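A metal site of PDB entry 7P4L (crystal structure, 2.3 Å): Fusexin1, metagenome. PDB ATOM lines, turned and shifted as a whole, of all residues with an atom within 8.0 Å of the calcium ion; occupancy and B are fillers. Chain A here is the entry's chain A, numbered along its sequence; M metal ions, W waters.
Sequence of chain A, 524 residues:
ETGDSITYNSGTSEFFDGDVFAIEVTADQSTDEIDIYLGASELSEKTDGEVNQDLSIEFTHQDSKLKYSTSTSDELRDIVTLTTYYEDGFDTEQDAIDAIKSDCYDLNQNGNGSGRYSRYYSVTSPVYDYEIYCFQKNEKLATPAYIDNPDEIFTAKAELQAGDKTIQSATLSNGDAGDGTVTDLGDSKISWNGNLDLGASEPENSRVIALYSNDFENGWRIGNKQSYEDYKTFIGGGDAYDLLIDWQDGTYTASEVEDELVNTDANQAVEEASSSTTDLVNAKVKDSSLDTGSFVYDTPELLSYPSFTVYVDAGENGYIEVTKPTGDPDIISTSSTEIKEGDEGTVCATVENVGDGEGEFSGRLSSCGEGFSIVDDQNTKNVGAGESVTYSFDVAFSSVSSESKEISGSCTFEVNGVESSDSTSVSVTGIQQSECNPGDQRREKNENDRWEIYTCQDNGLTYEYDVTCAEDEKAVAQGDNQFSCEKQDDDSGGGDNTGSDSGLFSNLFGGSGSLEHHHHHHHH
OG of Ser 122 sits at hydrogen-bond distance from N of Ser 125, 3.1 Å away. The backbone NH of Tyr 120 sits at hydrogen-bond distance from the backbone carbonyl oxygen of Asp 129, 2.8 Å away.
Four residues have an atom within 4 Å of the calcium ion: Asp 91, Ser 125, Tyr 128 and Asp 129. The nearest printed residue that does not touch the calcium ion is Pro 126 (4.1 Å).
The calcium ion is bound by OD1 of Asp 91, O of Tyr 128, OG of Ser 125, O of Ser 125, water W1, OD1 of Asp 129 and O of Asp 91.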
ATOM      1  N   GLY A  89     -24.390   3.055 -15.839  1.00  0.00           N
ATOM      2  CA  GLY A  89     -24.638   3.827 -14.646  1.00  0.00           C
ATOM      3  C   GLY A  89     -23.456   4.596 -14.113  1.00  0.00           C
ATOM      4  O   GLY A  89     -23.576   5.220 -13.050  1.00  0.00           O
ATOM      5  N   PHE A  90     -22.309   4.548 -14.788  1.00  0.00           N
ATOM      6  CA  PHE A  90     -21.155   5.316 -14.333  1.00  0.00           C
ATOM      7  C   PHE A  90     -21.419   6.803 -14.564  1.00  0.00           C
ATOM      8  O   PHE A  90     -21.900   7.198 -15.633  1.00  0.00           O
ATOM      9  CB  PHE A  90     -19.897   4.870 -15.069  1.00  0.00           C
ATOM     10  CG  PHE A  90     -19.526   3.429 -14.801  1.00  0.00           C
ATOM     11  CD1 PHE A  90     -18.852   3.079 -13.645  1.00  0.00           C
ATOM     12  CD2 PHE A  90     -19.848   2.431 -15.712  1.00  0.00           C
ATOM     13  CE1 PHE A  90     -18.514   1.769 -13.391  1.00  0.00           C
ATOM     14  CE2 PHE A  90     -19.505   1.112 -15.456  1.00  0.00           C
ATOM     15  CZ  PHE A  90     -18.833   0.784 -14.300  1.00  0.00           C
ATOM     16  N   ASP A  91     -21.115   7.623 -13.561  1.00  0.00           N
ATOM     17  CA  ASP A  91     -21.452   9.047 -13.627  1.00  0.00           C
ATOM     18  C   ASP A  91     -20.504   9.805 -14.553  1.00  0.00           C
ATOM     19  O   ASP A  91     -20.957  10.608 -15.375  1.00  0.00           O
ATOM     20  CB  ASP A  91     -21.404   9.656 -12.228  1.00  0.00           C
ATOM     21  CG  ASP A  91     -21.836  11.124 -12.221  1.00  0.00           C
ATOM     22  OD1 ASP A  91     -22.473  11.574 -13.201  1.00  0.00           O
ATOM     23  OD2 ASP A  91     -21.538  11.822 -11.225  1.00  0.00           O
ATOM     24  N   THR A  92     -19.206   9.554 -14.441  1.00  0.00           N
ATOM     25  CA  THR A  92     -18.210  10.288 -15.204  1.00  0.00           C
ATOM     26  C   THR A  92     -17.314   9.322 -15.970  1.00  0.00           C
ATOM     27  O   THR A  92     -17.245   8.133 -15.679  1.00  0.00           O
ATOM     28  CB  THR A  92     -17.344  11.173 -14.287  1.00  0.00           C
ATOM     29  OG1 THR A  92     -16.619  10.346 -13.373  1.00  0.00           O
ATOM     30  CG2 THR A  92     -18.218  12.141 -13.516  1.00  0.00           C
ATOM     31  N   GLU A  93     -16.622   9.881 -16.961  1.00  0.00           N
ATOM     32  CA  GLU A  93     -15.678   9.095 -17.751  1.00  0.00           C
ATOM     33  C   GLU A  93     -14.594   8.497 -16.869  1.00  0.00           C
ATOM     34  O   GLU A  93     -14.180   7.354 -17.053  1.00  0.00           O
ATOM     35  CB  GLU A  93     -15.072   9.980 -18.843  1.00  0.00           C
ATOM     36  CG  GLU A  93     -14.046   9.316 -19.742  1.00  0.00           C
ATOM     37  CD  GLU A  93     -13.567  10.251 -20.840  1.00  0.00           C
ATOM     38  OE1 GLU A  93     -13.937  11.441 -20.809  1.00  0.00           O
ATOM     39  OE2 GLU A  93     -12.833   9.797 -21.737  1.00  0.00           O
ATOM     40  N   ASP A  95     -14.870   7.634 -13.762  1.00  0.00           N
ATOM     41  CA  ASP A  95     -15.462   6.496 -13.046  1.00  0.00           C
ATOM     42  C   ASP A  95     -15.412   5.237 -13.902  1.00  0.00           C
ATOM     43  O   ASP A  95     -15.045   4.156 -13.427  1.00  0.00           O
ATOM     44  CB  ASP A  95     -16.905   6.815 -12.654  1.00  0.00           C
ATOM     45  CG  ASP A  95     -16.996   7.947 -11.648  1.00  0.00           C
ATOM     46  OD1 ASP A  95     -15.997   8.220 -10.959  1.00  0.00           O
ATOM     47  OD2 ASP A  95     -18.079   8.563 -11.564  1.00  0.00           O
ATOM     48  N   TYR A 120     -23.303   8.239 -22.903  1.00  0.00           N
ATOM     49  CA  TYR A 120     -24.665   8.377 -23.392  1.00  0.00           C
ATOM     50  C   TYR A 120     -25.368   9.506 -22.648  1.00  0.00           C
ATOM     51  O   TYR A 120     -25.103   9.767 -21.470  1.00  0.00           O
ATOM     52  CB  TYR A 120     -25.465   7.074 -23.262  1.00  0.00           C
ATOM     53  CG  TYR A 120     -25.539   6.476 -21.875  1.00  0.00           C
ATOM     54  CD1 TYR A 120     -24.501   5.717 -21.369  1.00  0.00           C
ATOM     55  CD2 TYR A 120     -26.667   6.654 -21.078  1.00  0.00           C
ATOM     56  CE1 TYR A 120     -24.569   5.157 -20.102  1.00  0.00           C
ATOM     57  CE2 TYR A 120     -26.741   6.103 -19.812  1.00  0.00           C
ATOM     58  CZ  TYR A 120     -25.684   5.364 -19.332  1.00  0.00           C
ATOM     59  OH  TYR A 120     -25.735   4.802 -18.082  1.00  0.00           O
ATOM     60  N   TYR A 121     -26.280  10.168 -23.365  1.00  0.00           N
ATOM     61  CA  TYR A 121     -26.995  11.317 -22.818  1.00  0.00           C
ATOM     62  C   TYR A 121     -27.787  10.897 -21.587  1.00  0.00           C
ATOM     63  O   TYR A 121     -28.501   9.879 -21.612  1.00  0.00           O
ATOM     64  CB  TYR A 121     -27.915  11.889 -23.899  1.00  0.00           C
ATOM     65  CG  TYR A 121     -28.583  13.198 -23.561  1.00  0.00           C
ATOM     66  CD1 TYR A 121     -27.857  14.379 -23.517  1.00  0.00           C
ATOM     67  CD2 TYR A 121     -29.959  13.261 -23.318  1.00  0.00           C
ATOM     68  CE1 TYR A 121     -28.465  15.591 -23.221  1.00  0.00           C
ATOM     69  CE2 TYR A 121     -30.577  14.468 -23.014  1.00  0.00           C
ATOM     70  CZ  TYR A 121     -29.820  15.620 -22.974  1.00  0.00           C
ATOM     71  OH  TYR A 121     -30.423  16.824 -22.676  1.00  0.00           O
ATOM     72  N   SER A 122     -27.653  11.668 -20.512  1.00  0.00           N
ATOM     73  CA  SER A 122     -28.307  11.374 -19.235  1.00  0.00           C
ATOM     74  C   SER A 122     -28.983  12.626 -18.717  1.00  0.00           C
ATOM     75  O   SER A 122     -28.307  13.618 -18.383  1.00  0.00           O
ATOM     76  CB  SER A 122     -27.290  10.830 -18.224  1.00  0.00           C
ATOM     77  OG  SER A 122     -27.893  10.528 -16.986  1.00  0.00           O
ATOM     78  N   VAL A 123     -30.320  12.614 -18.631  1.00  0.00           N
ATOM     79  CA  VAL A 123     -31.034  13.744 -18.044  1.00  0.00           C
ATOM     80  C   VAL A 123     -30.819  13.784 -16.536  1.00  0.00           C
ATOM     81  O   VAL A 123     -30.690  14.867 -15.944  1.00  0.00           O
ATOM     82  CB  VAL A 123     -32.529  13.697 -18.396  1.00  0.00           C
ATOM     83  CG1 VAL A 123     -32.732  13.829 -19.905  1.00  0.00           C
ATOM     84  CG2 VAL A 123     -33.187  12.415 -17.874  1.00  0.00           C
ATOM     85  N   THR A 124     -30.777  12.615 -15.893  1.00  0.00           N
ATOM     86  CA  THR A 124     -30.706  12.561 -14.442  1.00  0.00           C
ATOM     87  C   THR A 124     -29.312  12.893 -13.928  1.00  0.00           C
ATOM     88  O   THR A 124     -29.165  13.517 -12.866  1.00  0.00           O
ATOM     89  CB  THR A 124     -31.130  11.173 -13.953  1.00  0.00           C
ATOM     90  OG1 THR A 124     -32.517  10.960 -14.266  1.00  0.00           O
ATOM     91  CG2 THR A 124     -30.910  11.038 -12.451  1.00  0.00           C
ATOM     92  N   SER A 125     -28.272  12.502 -14.660  1.00  0.00           N
ATOM     93  CA  SER A 125     -26.881  12.782 -14.292  1.00  0.00           C
ATOM     94  C   SER A 125     -26.202  13.428 -15.500  1.00  0.00           C
ATOM     95  O   SER A 125     -25.342  12.830 -16.147  1.00  0.00           O
ATOM     96  CB  SER A 125     -26.165  11.498 -13.869  1.00  0.00           C
ATOM     97  OG  SER A 125     -24.851  11.756 -13.376  1.00  0.00           O
ATOM     98  N   PRO A 126     -26.591  14.653 -15.820  1.00  0.00           N
ATOM     99  CA  PRO A 126     -26.076  15.292 -17.034  1.00  0.00           C
ATOM    100  C   PRO A 126     -24.615  15.699 -16.882  1.00  0.00           C
ATOM    101  O   PRO A 126     -24.098  15.860 -15.773  1.00  0.00           O
ATOM    102  CB  PRO A 126     -26.980  16.509 -17.215  1.00  0.00           C
ATOM    103  CG  PRO A 126     -27.439  16.839 -15.840  1.00  0.00           C
ATOM    104  CD  PRO A 126     -27.528  15.530 -15.098  1.00  0.00           C
ATOM    105  N   VAL A 127     -23.938  15.881 -18.014  1.00  0.00           N
ATOM    106  CA  VAL A 127     -24.520  15.704 -19.354  1.00  0.00           C
ATOM    107  C   VAL A 127     -24.597  14.223 -19.764  1.00  0.00           C
ATOM    108  O   VAL A 127     -25.513  13.833 -20.490  1.00  0.00           O
ATOM    109  CB  VAL A 127     -23.731  16.493 -20.397  1.00  0.00           C
ATOM    110  CG1 VAL A 127     -24.347  16.326 -21.775  1.00  0.00           C
ATOM    111  CG2 VAL A 127     -23.666  17.963 -20.010  1.00  0.00           C
ATOM    112  N   TYR A 128     -23.642  13.421 -19.300  1.00  0.00           N
ATOM    113  CA  TYR A 128     -23.539  12.026 -19.728  1.00  0.00           C
ATOM    114  C   TYR A 128     -23.398  11.092 -18.540  1.00  0.00           C
ATOM    115  O   TYR A 128     -22.928  11.492 -17.464  1.00  0.00           O
ATOM    116  CB  TYR A 128     -22.338  11.820 -20.653  1.00  0.00           C
ATOM    117  CG  TYR A 128     -22.345  12.678 -21.895  1.00  0.00           C
ATOM    118  CD1 TYR A 128     -23.102  12.323 -23.004  1.00  0.00           C
ATOM    119  CD2 TYR A 128     -21.565  13.821 -21.973  1.00  0.00           C
ATOM    120  CE1 TYR A 128     -23.111  13.107 -24.147  1.00  0.00           C
ATOM    121  CE2 TYR A 128     -21.565  14.611 -23.114  1.00  0.00           C
ATOM    122  CZ  TYR A 128     -22.337  14.249 -24.196  1.00  0.00           C
ATOM    123  OH  TYR A 128     -22.334  15.030 -25.326  1.00  0.00           O
ATOM    124  N   ASP A 129     -23.841   9.856 -18.747  1.00  0.00           N
ATOM    125  CA  ASP A 129     -23.381   8.682 -18.019  1.00  0.00           C
ATOM    126  C   ASP A 129     -22.589   7.808 -18.990  1.00  0.00           C
ATOM    127  O   ASP A 129     -22.520   8.092 -20.185  1.00  0.00           O
ATOM    128  CB  ASP A 129     -24.547   7.911 -17.400  1.00  0.00           C
ATOM    129  CG  ASP A 129     -25.012   8.516 -16.077  1.00  0.00           C
ATOM    130  OD1 ASP A 129     -24.416   9.517 -15.638  1.00  0.00           O
ATOM    131  OD2 ASP A 129     -25.974   7.986 -15.484  1.00  0.00           O
ATOM    132  N   TYR A 130     -22.001   6.726 -18.475  1.00  0.00           N
ATOM    133  CA  TYR A 130     -21.046   5.959 -19.261  1.00  0.00           C
ATOM    134  C   TYR A 130     -21.274   4.456 -19.112  1.00  0.00           C
ATOM    135  O   TYR A 130     -21.569   3.975 -18.017  1.00  0.00           O
ATOM    136  CB  TYR A 130     -19.612   6.306 -18.850  1.00  0.00           C
ATOM    137  CG  TYR A 130     -19.232   7.728 -19.204  1.00  0.00           C
ATOM    138  CD1 TYR A 130     -19.675   8.797 -18.424  1.00  0.00           C
ATOM    139  CD2 TYR A 130     -18.479   8.016 -20.326  1.00  0.00           C
ATOM    140  CE1 TYR A 130     -19.358  10.091 -18.735  1.00  0.00           C
ATOM    141  CE2 TYR A 130     -18.149   9.316 -20.654  1.00  0.00           C
ATOM    142  CZ  TYR A 130     -18.598  10.348 -19.856  1.00  0.00           C
ATOM    143  OH  TYR A 130     -18.277  11.656 -20.166  1.00  0.00           O
HETATM  144 CA    CA M   1     -23.356  11.826 -15.209  1.00  0.00          CA
HETATM  145  O   HOH W   1     -21.974  13.970 -15.452  1.00  0.00           O
